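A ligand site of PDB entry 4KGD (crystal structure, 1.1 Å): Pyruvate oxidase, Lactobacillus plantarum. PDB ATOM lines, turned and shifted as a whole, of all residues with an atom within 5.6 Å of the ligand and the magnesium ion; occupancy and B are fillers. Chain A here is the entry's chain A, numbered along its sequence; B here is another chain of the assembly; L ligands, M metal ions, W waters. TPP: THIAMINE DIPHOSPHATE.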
ATOM      1  N   ASN A  92      13.996  18.738 -11.705  1.00  0.00           N
ATOM      2  CA  ASN A  92      13.561  19.572 -10.592  1.00  0.00           C
ATOM      3  C   ASN A  92      13.447  18.756  -9.310  1.00  0.00           C
ATOM      4  O   ASN A  92      13.654  19.285  -8.212  1.00  0.00           O
ATOM      5  CB  ASN A  92      12.272  20.321 -10.874  1.00  0.00           C
ATOM      6  CG  ASN A  92      12.578  21.530 -11.712  1.00  0.00           C
ATOM      7  OD1 ASN A  92      13.296  21.462 -12.696  1.00  0.00           O
ATOM      8  ND2 ASN A  92      12.072  22.687 -11.306  1.00  0.00           N
ATOM      9  N   ASP A 393       3.305  23.449  -1.383  1.00  0.00           N
ATOM     10  CA  ASP A 393       3.949  23.936  -2.598  1.00  0.00           C
ATOM     11  C   ASP A 393       4.767  25.191  -2.234  1.00  0.00           C
ATOM     12  O   ASP A 393       5.124  25.401  -1.084  1.00  0.00           O
ATOM     13  CB  ASP A 393       2.904  24.134  -3.715  1.00  0.00           C
ATOM     14  CG  ASP A 393       3.486  23.866  -5.098  1.00  0.00           C
ATOM     15  OD1 ASP A 393       4.270  24.674  -5.606  1.00  0.00           O
ATOM     16  OD2 ASP A 393       3.114  22.790  -5.666  1.00  0.00           O
ATOM     17  N   VAL A 394       5.091  26.020  -3.255  1.00  0.00           N
ATOM     18  CA  VAL A 394       6.054  27.123  -3.090  1.00  0.00           C
ATOM     19  C   VAL A 394       5.382  28.417  -3.507  1.00  0.00           C
ATOM     20  O   VAL A 394       4.865  28.534  -4.639  1.00  0.00           O
ATOM     21  CB  VAL A 394       7.326  26.849  -3.906  1.00  0.00           C
ATOM     22  CG1 VAL A 394       8.233  28.072  -3.994  1.00  0.00           C
ATOM     23  CG2 VAL A 394       8.042  25.664  -3.308  1.00  0.00           C
ATOM     24  N   GLY A 395       5.422  29.421  -2.618  1.00  0.00           N
ATOM     25  CA  GLY A 395       4.840  30.721  -2.872  1.00  0.00           C
ATOM     26  C   GLY A 395       4.258  31.297  -1.598  1.00  0.00           C
ATOM     27  O   GLY A 395       4.709  30.973  -0.495  1.00  0.00           O
ATOM     28  N   ASP A 396       3.222  32.130  -1.755  1.00  0.00           N
ATOM     29  CA  ASP A 396       2.577  32.656  -0.575  1.00  0.00           C
ATOM     30  C   ASP A 396       2.115  31.541   0.374  1.00  0.00           C
ATOM     31  O   ASP A 396       2.043  31.797   1.579  1.00  0.00           O
ATOM     32  CB  ASP A 396       1.403  33.530  -0.935  1.00  0.00           C
ATOM     33  CG  ASP A 396       1.664  34.929  -1.372  1.00  0.00           C
ATOM     34  OD1 ASP A 396       2.750  35.453  -1.136  1.00  0.00           O
ATOM     35  OD2 ASP A 396       0.682  35.554  -1.892  1.00  0.00           O
ATOM     36  N   ILE A 397       1.779  30.358  -0.112  1.00  0.00           N
ATOM     37  CA  ILE A 397       1.369  29.309   0.803  1.00  0.00           C
ATOM     38  C   ILE A 397       2.410  28.997   1.839  1.00  0.00           C
ATOM     39  O   ILE A 397       2.030  28.636   2.970  1.00  0.00           O
ATOM     40  CB  ILE A 397       0.930  28.032   0.042  1.00  0.00           C
ATOM     41  CG1 ILE A 397       0.211  27.040   0.945  1.00  0.00           C
ATOM     42  CG2 ILE A 397       2.080  27.355  -0.705  1.00  0.00           C
ATOM     43  CD1 ILE A 397      -0.994  27.568   1.686  1.00  0.00           C
ATOM     44  N   PHE A 419      15.899  24.429  -2.673  1.00  0.00           N
ATOM     45  CA  PHE A 419      15.753  24.596  -4.117  1.00  0.00           C
ATOM     46  C   PHE A 419      14.445  25.342  -4.442  1.00  0.00           C
ATOM     47  O   PHE A 419      14.335  26.048  -5.456  1.00  0.00           O
ATOM     48  CB  PHE A 419      15.803  23.226  -4.799  1.00  0.00           C
ATOM     49  CG  PHE A 419      15.964  23.286  -6.312  1.00  0.00           C
ATOM     50  CD1 PHE A 419      17.062  23.885  -6.893  1.00  0.00           C
ATOM     51  CD2 PHE A 419      15.015  22.664  -7.128  1.00  0.00           C
ATOM     52  CE1 PHE A 419      17.211  23.873  -8.271  1.00  0.00           C
ATOM     53  CE2 PHE A 419      15.175  22.680  -8.509  1.00  0.00           C
ATOM     54  CZ  PHE A 419      16.262  23.276  -9.055  1.00  0.00           C
ATOM     55  N   ALA A 420      13.439  25.147  -3.616  1.00  0.00           N
ATOM     56  CA  ALA A 420      12.158  25.819  -3.678  1.00  0.00           C
ATOM     57  C   ALA A 420      11.533  25.678  -5.076  1.00  0.00           C
ATOM     58  O   ALA A 420      11.021  26.632  -5.652  1.00  0.00           O
ATOM     59  CB  ALA A 420      12.252  27.286  -3.262  1.00  0.00           C
ATOM     60  N   THR A 421      11.476  24.437  -5.565  1.00  0.00           N
ATOM     61  CA  THR A 421      10.758  24.181  -6.788  1.00  0.00           C
ATOM     62  C   THR A 421       9.237  24.185  -6.563  1.00  0.00           C
ATOM     63  O   THR A 421       8.704  23.409  -5.788  1.00  0.00           O
ATOM     64  CB  THR A 421      11.220  22.909  -7.509  1.00  0.00           C
ATOM     65  OG1 THR A 421      10.486  22.803  -8.740  1.00  0.00           O
ATOM     66  CG2 THR A 421      11.063  21.649  -6.710  1.00  0.00           C
ATOM     67  N   MET A 422       8.543  25.061  -7.322  1.00  0.00           N
ATOM     68  CA  MET A 422       7.119  24.958  -7.427  1.00  0.00           C
ATOM     69  C   MET A 422       6.728  23.598  -7.996  1.00  0.00           C
ATOM     70  O   MET A 422       7.520  22.970  -8.725  1.00  0.00           O
ATOM     71  CB  MET A 422       6.580  26.043  -8.336  1.00  0.00           C
ATOM     72  CG  MET A 422       6.683  27.472  -7.795  1.00  0.00           C
ATOM     73  SD  MET A 422       6.439  28.707  -9.038  1.00  0.00           S
ATOM     74  CE  MET A 422       4.739  28.415  -9.487  1.00  0.00           C
ATOM     75  N   ALA A 445      -1.444  24.247  -2.071  1.00  0.00           N
ATOM     76  CA  ALA A 445      -0.708  24.777  -3.248  1.00  0.00           C
ATOM     77  C   ALA A 445      -1.361  26.039  -3.768  1.00  0.00           C
ATOM     78  O   ALA A 445      -2.578  26.158  -3.854  1.00  0.00           O
ATOM     79  CB  ALA A 445      -0.689  23.743  -4.354  1.00  0.00           C
ATOM     80  N   GLY A 446      -0.513  26.981  -4.191  1.00  0.00           N
ATOM     81  CA  GLY A 446      -0.992  28.066  -5.007  1.00  0.00           C
ATOM     82  C   GLY A 446      -1.386  27.627  -6.411  1.00  0.00           C
ATOM     83  O   GLY A 446      -1.008  26.535  -6.845  1.00  0.00           O
ATOM     84  N   ASP A 447      -2.101  28.483  -7.097  1.00  0.00           N
ATOM     85  CA  ASP A 447      -2.551  28.157  -8.449  1.00  0.00           C
ATOM     86  C   ASP A 447      -1.385  28.018  -9.427  1.00  0.00           C
ATOM     87  O   ASP A 447      -1.411  27.157 -10.316  1.00  0.00           O
ATOM     88  CB  ASP A 447      -3.593  29.125  -8.960  1.00  0.00           C
ATOM     89  CG  ASP A 447      -3.359  30.630  -8.833  1.00  0.00           C
ATOM     90  OD1 ASP A 447      -2.315  31.057  -8.303  1.00  0.00           O
ATOM     91  OD2 ASP A 447      -4.257  31.374  -9.279  1.00  0.00           O
ATOM     92  N   GLY A 448      -0.351  28.839  -9.298  1.00  0.00           N
ATOM     93  CA  GLY A 448       0.796  28.705 -10.170  1.00  0.00           C
ATOM     94  C   GLY A 448       1.517  27.386  -9.993  1.00  0.00           C
ATOM     95  O   GLY A 448       1.836  26.697 -10.978  1.00  0.00           O
ATOM     96  N   GLY A 449       1.725  26.963  -8.744  1.00  0.00           N
ATOM     97  CA  GLY A 449       2.419  25.719  -8.467  1.00  0.00           C
ATOM     98  C   GLY A 449       1.582  24.504  -8.785  1.00  0.00           C
ATOM     99  O   GLY A 449       2.063  23.521  -9.386  1.00  0.00           O
ATOM    100  N   ALA A 450       0.313  24.535  -8.415  1.00  0.00           N
ATOM    101  CA  ALA A 450      -0.610  23.448  -8.759  1.00  0.00           C
ATOM    102  C   ALA A 450      -0.666  23.267 -10.254  1.00  0.00           C
ATOM    103  O   ALA A 450      -0.749  22.141 -10.740  1.00  0.00           O
ATOM    104  CB  ALA A 450      -1.993  23.706  -8.218  1.00  0.00           C
ATOM    105  N   MET A 452       1.607  23.695 -12.436  1.00  0.00           N
ATOM    106  CA  MET A 452       2.798  23.059 -12.981  1.00  0.00           C
ATOM    107  C   MET A 452       2.734  21.559 -12.932  1.00  0.00           C
ATOM    108  O   MET A 452       3.335  20.927 -13.824  1.00  0.00           O
ATOM    109  CB  MET A 452       4.084  23.560 -12.267  1.00  0.00           C
ATOM    110  CG  MET A 452       4.396  24.995 -12.687  1.00  0.00           C
ATOM    111  SD  MET A 452       5.894  25.548 -11.901  1.00  0.00           S
ATOM    112  CE  MET A 452       6.041  27.158 -12.686  1.00  0.00           C
ATOM    113  N   PHE A 472      -5.049  27.536  -3.882  1.00  0.00           N
ATOM    114  CA  PHE A 472      -5.237  28.936  -3.515  1.00  0.00           C
ATOM    115  C   PHE A 472      -5.203  29.760  -4.804  1.00  0.00           C
ATOM    116  O   PHE A 472      -4.143  30.099  -5.303  1.00  0.00           O
ATOM    117  CB  PHE A 472      -4.202  29.418  -2.500  1.00  0.00           C
ATOM    118  CG  PHE A 472      -4.332  28.730  -1.153  1.00  0.00           C
ATOM    119  CD1 PHE A 472      -4.071  27.395  -0.923  1.00  0.00           C
ATOM    120  CD2 PHE A 472      -4.779  29.484  -0.053  1.00  0.00           C
ATOM    121  CE1 PHE A 472      -4.238  26.794   0.288  1.00  0.00           C
ATOM    122  CE2 PHE A 472      -4.896  28.906   1.177  1.00  0.00           C
ATOM    123  CZ  PHE A 472      -4.665  27.560   1.372  1.00  0.00           C
ATOM    124  N   THR A 473      -6.386  30.040  -5.353  1.00  0.00           N
ATOM    125  CA  THR A 473      -6.477  30.694  -6.668  1.00  0.00           C
ATOM    126  C   THR A 473      -6.593  32.177  -6.516  1.00  0.00           C
ATOM    127  O   THR A 473      -7.678  32.696  -6.194  1.00  0.00           O
ATOM    128  CB  THR A 473      -7.616  30.077  -7.499  1.00  0.00           C
ATOM    129  OG1 THR A 473      -7.215  28.754  -7.825  1.00  0.00           O
ATOM    130  CG2 THR A 473      -7.843  30.892  -8.751  1.00  0.00           C
ATOM    131  N   ASN A 474      -5.462  32.884  -6.724  1.00  0.00           N
ATOM    132  CA  ASN A 474      -5.439  34.332  -6.739  1.00  0.00           C
ATOM    133  C   ASN A 474      -5.254  34.875  -8.165  1.00  0.00           C
ATOM    134  O   ASN A 474      -5.248  36.096  -8.328  1.00  0.00           O
ATOM    135  CB  ASN A 474      -4.401  34.919  -5.806  1.00  0.00           C
ATOM    136  CG  ASN A 474      -3.049  34.305  -5.941  1.00  0.00           C
ATOM    137  OD1 ASN A 474      -2.719  33.644  -6.915  1.00  0.00           O
ATOM    138  ND2 ASN A 474      -2.181  34.554  -4.953  1.00  0.00           N
ATOM    139  N   CYS A 475      -5.100  34.011  -9.167  1.00  0.00           N
ATOM    140  CA  CYS A 475      -4.787  34.464 -10.534  1.00  0.00           C
ATOM    141  C   CYS A 475      -3.522  35.287 -10.606  1.00  0.00           C
ATOM    142  O   CYS A 475      -3.356  36.161 -11.424  1.00  0.00           O
ATOM    143  CB  CYS A 475      -5.956  35.189 -11.170  1.00  0.00           C
ATOM    144  SG  CYS A 475      -7.437  34.176 -11.364  1.00  0.00           S
ATOM    145  N   GLN A 476      -2.573  34.897  -9.739  1.00  0.00           N
ATOM    146  CA  GLN A 476      -1.301  35.599  -9.663  1.00  0.00           C
ATOM    147  C   GLN A 476      -0.189  34.644  -9.281  1.00  0.00           C
ATOM    148  O   GLN A 476      -0.430  33.599  -8.631  1.00  0.00           O
ATOM    149  CB  GLN A 476      -1.289  36.679  -8.583  1.00  0.00           C
ATOM    150  CG  GLN A 476      -2.369  37.723  -8.697  1.00  0.00           C
ATOM    151  CD  GLN A 476      -2.420  38.666  -7.510  1.00  0.00           C
ATOM    152  OE1 GLN A 476      -2.846  39.845  -7.654  1.00  0.00           O
ATOM    153  NE2 GLN A 476      -2.011  38.287  -6.402  1.00  0.00           N
ATOM    154  N   TYR A 477       1.013  35.038  -9.616  1.00  0.00           N
ATOM    155  CA  TYR A 477       2.221  34.588  -8.908  1.00  0.00           C
ATOM    156  C   TYR A 477       2.380  35.579  -7.755  1.00  0.00           C
ATOM    157  O   TYR A 477       3.170  36.554  -7.868  1.00  0.00           O
ATOM    158  CB  TYR A 477       3.440  34.562  -9.819  1.00  0.00           C
ATOM    159  CG  TYR A 477       3.370  33.564 -10.949  1.00  0.00           C
ATOM    160  CD1 TYR A 477       3.080  32.229 -10.731  1.00  0.00           C
ATOM    161  CD2 TYR A 477       3.612  33.977 -12.234  1.00  0.00           C
ATOM    162  CE1 TYR A 477       3.023  31.324 -11.786  1.00  0.00           C
ATOM    163  CE2 TYR A 477       3.534  33.072 -13.289  1.00  0.00           C
ATOM    164  CZ  TYR A 477       3.255  31.745 -13.064  1.00  0.00           C
ATOM    165  OH  TYR A 477       3.169  30.884 -14.109  1.00  0.00           O
ATOM    166  N   GLY A 478       1.587  35.450  -6.702  1.00  0.00           N
ATOM    167  CA  GLY A 478       1.498  36.476  -5.695  1.00  0.00           C
ATOM    168  C   GLY A 478       2.798  36.802  -5.035  1.00  0.00           C
ATOM    169  O   GLY A 478       3.192  37.946  -4.851  1.00  0.00           O
ATOM    170  N   PHE A 479       3.546  35.711  -4.695  1.00  0.00           N
ATOM    171  CA  PHE A 479       4.843  35.901  -4.044  1.00  0.00           C
ATOM    172  C   PHE A 479       5.759  36.803  -4.860  1.00  0.00           C
ATOM    173  O   PHE A 479       6.523  37.587  -4.315  1.00  0.00           O
ATOM    174  CB  PHE A 479       5.483  34.534  -3.804  1.00  0.00           C
ATOM    175  CG  PHE A 479       6.429  34.363  -2.654  1.00  0.00           C
ATOM    176  CD1 PHE A 479       5.982  34.449  -1.339  1.00  0.00           C
ATOM    177  CD2 PHE A 479       7.740  34.073  -2.900  1.00  0.00           C
ATOM    178  CE1 PHE A 479       6.906  34.240  -0.299  1.00  0.00           C
ATOM    179  CE2 PHE A 479       8.635  33.862  -1.887  1.00  0.00           C
ATOM    180  CZ  PHE A 479       8.197  33.926  -0.577  1.00  0.00           C
ATOM    181  N   ILE A 480       5.713  36.617  -6.178  1.00  0.00           N
ATOM    182  CA  ILE A 480       6.557  37.405  -7.089  1.00  0.00           C
ATOM    183  C   ILE A 480       5.977  38.779  -7.386  1.00  0.00           C
ATOM    184  O   ILE A 480       6.765  39.740  -7.498  1.00  0.00           O
ATOM    185  CB  ILE A 480       6.794  36.642  -8.408  1.00  0.00           C
ATOM    186  CG1 ILE A 480       7.282  35.225  -8.149  1.00  0.00           C
ATOM    187  CG2 ILE A 480       7.766  37.414  -9.304  1.00  0.00           C
ATOM    188  CD1 ILE A 480       8.450  35.138  -7.235  1.00  0.00           C
ATOM    189  N   PHE A 497      -2.461  36.717 -14.168  1.00  0.00           N
ATOM    190  CA  PHE A 497      -2.777  35.853 -15.311  1.00  0.00           C
ATOM    191  C   PHE A 497      -4.231  35.406 -15.233  1.00  0.00           C
ATOM    192  O   PHE A 497      -4.971  35.727 -14.289  1.00  0.00           O
ATOM    193  CB  PHE A 497      -1.781  34.680 -15.369  1.00  0.00           C
ATOM    194  CG  PHE A 497      -1.553  33.916 -14.115  1.00  0.00           C
ATOM    195  CD1 PHE A 497      -2.586  33.154 -13.496  1.00  0.00           C
ATOM    196  CD2 PHE A 497      -0.322  33.920 -13.487  1.00  0.00           C
ATOM    197  CE1 PHE A 497      -2.297  32.433 -12.360  1.00  0.00           C
ATOM    198  CE2 PHE A 497      -0.043  33.193 -12.343  1.00  0.00           C
ATOM    199  CZ  PHE A 497      -1.045  32.476 -11.765  1.00  0.00           C
ATOM    200  N   ILE B  32       8.745  32.730 -16.925  1.00  0.00           N
ATOM    201  CA  ILE B  32       7.992  32.958 -15.708  1.00  0.00           C
ATOM    202  C   ILE B  32       8.887  33.794 -14.820  1.00  0.00           C
ATOM    203  O   ILE B  32      10.069  33.477 -14.651  1.00  0.00           O
ATOM    204  CB  ILE B  32       7.632  31.613 -15.034  1.00  0.00           C
ATOM    205  CG1 ILE B  32       6.580  30.886 -15.876  1.00  0.00           C
ATOM    206  CG2 ILE B  32       7.148  31.791 -13.594  1.00  0.00           C
ATOM    207  CD1 ILE B  32       6.238  29.476 -15.423  1.00  0.00           C
ATOM    208  N   PRO B  33       8.360  34.882 -14.251  1.00  0.00           N
ATOM    209  CA  PRO B  33       9.227  35.768 -13.439  1.00  0.00           C
ATOM    210  C   PRO B  33       9.558  35.117 -12.089  1.00  0.00           C
ATOM    211  O   PRO B  33       8.951  34.201 -11.613  1.00  0.00           O
ATOM    212  CB  PRO B  33       8.363  37.011 -13.281  1.00  0.00           C
ATOM    213  CG  PRO B  33       6.976  36.453 -13.228  1.00  0.00           C
ATOM    214  CD  PRO B  33       6.973  35.353 -14.285  1.00  0.00           C
ATOM    215  N   GLY B  34      10.566  35.703 -11.468  1.00  0.00           N
ATOM    216  CA  GLY B  34      11.008  35.395 -10.132  1.00  0.00           C
ATOM    217  C   GLY B  34      11.872  36.535  -9.629  1.00  0.00           C
ATOM    218  O   GLY B  34      12.376  37.337 -10.435  1.00  0.00           O
ATOM    219  N   GLU B  59       7.962  26.541 -17.285  1.00  0.00           N
ATOM    220  CA  GLU B  59       9.086  27.011 -18.088  1.00  0.00           C
ATOM    221  C   GLU B  59       9.517  26.049 -19.203  1.00  0.00           C
ATOM    222  O   GLU B  59      10.080  26.511 -20.195  1.00  0.00           O
ATOM    223  CB  GLU B  59      10.306  27.338 -17.222  1.00  0.00           C
ATOM    224  CG  GLU B  59      10.058  28.402 -16.161  1.00  0.00           C
ATOM    225  CD  GLU B  59       9.543  27.881 -14.829  1.00  0.00           C
ATOM    226  OE1 GLU B  59       9.059  26.731 -14.736  1.00  0.00           O
ATOM    227  OE2 GLU B  59       9.598  28.699 -13.873  1.00  0.00           O
ATOM    228  N   SER B  82      13.784  31.547 -13.933  1.00  0.00           N
ATOM    229  CA  SER B  82      14.309  32.046 -12.684  1.00  0.00           C
ATOM    230  C   SER B  82      15.351  31.077 -12.108  1.00  0.00           C
ATOM    231  O   SER B  82      15.456  29.875 -12.445  1.00  0.00           O
ATOM    232  CB  SER B  82      13.114  32.232 -11.732  1.00  0.00           C
ATOM    233  OG  SER B  82      12.417  30.984 -11.478  1.00  0.00           O
ATOM    234  N   PRO B  85      15.060  26.262  -9.920  1.00  0.00           N
ATOM    235  CA  PRO B  85      14.036  25.480 -10.586  1.00  0.00           C
ATOM    236  C   PRO B  85      13.433  26.086 -11.823  1.00  0.00           C
ATOM    237  O   PRO B  85      12.831  25.350 -12.622  1.00  0.00           O
ATOM    238  CB  PRO B  85      12.961  25.309  -9.471  1.00  0.00           C
ATOM    239  CG  PRO B  85      13.196  26.480  -8.557  1.00  0.00           C
ATOM    240  CD  PRO B  85      14.700  26.596  -8.517  1.00  0.00           C
ATOM    241  N   GLY B  86      13.412  27.395 -11.966  1.00  0.00           N
ATOM    242  CA  GLY B  86      12.898  27.969 -13.215  1.00  0.00           C
ATOM    243  C   GLY B  86      13.754  27.507 -14.401  1.00  0.00           C
ATOM    244  O   GLY B  86      13.249  27.031 -15.412  1.00  0.00           O
ATOM    245  N   HIS B  89      13.712  23.737 -15.230  1.00  0.00           N
ATOM    246  CA  HIS B  89      12.521  23.399 -15.989  1.00  0.00           C
ATOM    247  C   HIS B  89      12.687  23.607 -17.509  1.00  0.00           C
ATOM    248  O   HIS B  89      11.889  23.044 -18.261  1.00  0.00           O
ATOM    249  CB  HIS B  89      11.324  24.166 -15.492  1.00  0.00           C
ATOM    250  CG  HIS B  89      10.483  23.481 -14.470  1.00  0.00           C
ATOM    251  ND1 HIS B  89       9.412  24.112 -13.874  1.00  0.00           N
ATOM    252  CD2 HIS B  89      10.405  22.189 -14.044  1.00  0.00           C
ATOM    253  CE1 HIS B  89       8.766  23.246 -13.112  1.00  0.00           C
ATOM    254  NE2 HIS B  89       9.352  22.064 -13.175  1.00  0.00           N
ATOM    255  N   GLN B 122      17.953  29.603  -2.635  1.00  0.00           N
ATOM    256  CA  GLN B 122      17.850  29.185  -4.029  1.00  0.00           C
ATOM    257  C   GLN B 122      19.094  29.649  -4.783  1.00  0.00           C
ATOM    258  O   GLN B 122      19.079  29.843  -5.995  1.00  0.00           O
ATOM    259  CB  GLN B 122      16.501  29.573  -4.532  1.00  0.00           C
ATOM    260  CG  GLN B 122      16.169  28.867  -5.882  1.00  0.00           C
ATOM    261  CD  GLN B 122      14.817  29.494  -6.124  1.00  0.00           C
ATOM    262  OE1 GLN B 122      13.845  28.760  -6.077  1.00  0.00           O
ATOM    263  NE2 GLN B 122      14.924  30.745  -6.454  1.00  0.00           N
HETATM  264  N1' TPP L   1       9.663  28.500 -11.253  1.00  0.00           N
HETATM  265  C2' TPP L   1       9.701  27.408 -10.491  1.00  0.00           C
HETATM  266  CM2 TPP L   1       9.542  26.096 -11.157  1.00  0.00           C
HETATM  267  N3' TPP L   1       9.923  27.468  -9.169  1.00  0.00           N
HETATM  268  C4' TPP L   1      10.081  28.716  -8.582  1.00  0.00           C
HETATM  269  N4' TPP L   1      10.392  28.744  -7.272  1.00  0.00           N
HETATM  270  C5' TPP L   1       9.895  29.884  -9.336  1.00  0.00           C
HETATM  271  C6' TPP L   1       9.741  29.785 -10.676  1.00  0.00           C
HETATM  272  C7' TPP L   1       9.866  31.271  -8.691  1.00  0.00           C
HETATM  273  N3  TPP L   1       8.672  31.471  -7.883  1.00  0.00           N
HETATM  274  C2  TPP L   1       8.790  31.403  -6.448  1.00  0.00           C
HETATM  275  S1  TPP L   1       7.197  31.645  -5.771  1.00  0.00           S
HETATM  276  C5  TPP L   1       6.515  31.941  -7.368  1.00  0.00           C
HETATM  277  C4  TPP L   1       7.412  31.837  -8.362  1.00  0.00           C
HETATM  278  CM4 TPP L   1       7.177  32.033  -9.838  1.00  0.00           C
HETATM  279  C6  TPP L   1       5.063  32.242  -7.492  1.00  0.00           C
HETATM  280  C7  TPP L   1       4.209  31.081  -6.977  1.00  0.00           C
HETATM  281  O7  TPP L   1       2.836  31.370  -7.484  1.00  0.00           O
HETATM  282  PA  TPP L   1       1.602  30.561  -6.896  1.00  0.00           P
HETATM  283  O1A TPP L   1       0.394  30.997  -7.666  1.00  0.00           O
HETATM  284  O2A TPP L   1       1.859  29.091  -6.879  1.00  0.00           O
HETATM  285  O3A TPP L   1       1.527  31.053  -5.395  1.00  0.00           O
HETATM  286  PB  TPP L   1       0.999  32.468  -4.751  1.00  0.00           P
HETATM  287  O1B TPP L   1       0.239  33.178  -5.856  1.00  0.00           O
HETATM  288  O2B TPP L   1       2.211  33.183  -4.278  1.00  0.00           O
HETATM  289  O3B TPP L   1       0.065  31.981  -3.634  1.00  0.00           O
HETATM  290 MG    MG M   1      -1.098  32.294  -7.221  1.00  0.00          MG
HETATM  291  O   HOH W   1      -1.788  31.273  -5.526  1.00  0.00           O
HETATM  292  O   HOH W   2      13.228  30.294  -9.011  1.00  0.00           O
HETATM  293  O   HOH W   3       2.228  27.659  -4.643  1.00  0.00           O
HETATM  294  O   HOH W   4      11.698  30.585  -5.511  1.00  0.00           O
HETATM  295  O   HOH W   5      10.435  31.828  -3.590  1.00  0.00           O
HETATM  296  O   HOH W   6       1.186  29.632  -2.752  1.00  0.00           O
HETATM  297  O   HOH W   7      -1.967  32.271  -1.801  1.00  0.00           O
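OE1 of Glu 59 of chain B sits at hydrogen-bond distance from ND1 of His 89 of chain B, at 2.8 Å.
N of Asp 447 is in hydrogen-bond range of O of Phe 472, 3.2 Å away.
A ring nitrogen (NE2) of His 89 of chain B sits close to the side-chain amide nitrogen (ND2) of Asn 92 (3.4 Å).
O of Phe 419 sits close to OE1 of Gln 122 of chain B, 2.8 Å away.
ND2 of Asn 92 sits at hydrogen-bond distance from O of Pro 85 of chain B (3.1 Å).
The side-chain carboxylate (OD2) of Asp 447 sits at hydrogen-bond distance from the backbone NH (N) of Cys 475 (2.8 Å).
An oxygen (O2A) of the ligand is in hydrogen-bond range of the backbone NH of Gly 448.
An oxygen (O2B) of the ligand sits at hydrogen-bond distance from the backbone NH (N) of Gly 478 (3.4 Å).
The backbone NH of Phe 479 sits at hydrogen-bond distance from an oxygen (O2B) of the ligand (2.9 Å).
The backbone carbonyl oxygen of Ala 420 sits at hydrogen-bond distance from a nitrogen (N4') of the ligand, at 2.7 Å.
The side-chain carboxylate (OE2) of Glu 59 of chain B sits at hydrogen-bond distance from a nitrogen (N1') of the ligand, 2.6 Å away.
N of Gly 449 is in hydrogen-bond range of O2A of the ligand (2.8 Å).
A nitrogen (N3') of the ligand lies within hydrogen-bond range of the backbone NH (N) of Met 422 (3.3 Å).
O2B of the ligand is in hydrogen-bond range of N of Asp 396 (2.9 Å).
The magnesium ion is bound by O1A of the ligand (2.0 Å), O of Gln 476 (2.0 Å), OD1 of Asp 447 (2.0 Å), water W1 (2.1 Å), O1B of the ligand (2.1 Å) and OD1 of Asn 474 (2.1 Å).
Of the 36 residues printed, 3 come within 4 Å of the magnesium ion.
The nearest printed residue that does not touch the magnesium ion is Gly 448 (4.1 Å).
Merely in contact with the ligand: Ser 82 of chain B (3.0 Å), Pro 33 of chain B (3.3 Å), His 89 of chain B (3.4 Å), Tyr 477 (3.4 Å), Ile 480 (3.4 Å), Pro 85 of chain B (3.5 Å), Val 394 (3.5 Å), Gly 446 (3.6 Å), Gln 122 of chain B (3.7 Å), Met 452 (3.8 Å), Ile 32 of chain B (3.8 Å), Gly 86 of chain B (3.8 Å) and Gly 395 (3.8 Å).
Hydrophobic or aromatic side chains within 4 Å of the ligand: Val 394, Met 422, Met 452, Tyr 477, Phe 479, Ile 480, Ile 32 of chain B, Pro 85 of chain B and His 89 of chain B.
Of the 36 residues printed, 24 come within 4 Å of the ligand.
The nearest printed residue that does not touch the ligand is Thr 421 (4.1 Å).
Water W1 lies within hydrogen-bond range of the backbone carbonyl oxygen (O) of Phe 472 (2.6 Å), an oxygen (O3B) of the ligand (2.7 Å), the backbone NH (N) of Asp 447 (3.2 Å) and the side-chain amide nitrogen (ND2) of Asn 474 (3.4 Å).
Water W3 lies within hydrogen-bond range of O2A of the ligand, O of Val 394 and N of Gly 446.
Water W4 bridges a nitrogen (N4') of the ligand (2.9 Å) and the side-chain amide oxygen (OE1) of Gln 122 of chain B (2.9 Å).
Water W2 lies within hydrogen-bond range of the side-chain hydroxyl of Ser 82 of chain B (2.7 Å) and the side-chain amide nitrogen of Gln 122 of chain B (3.1 Å).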
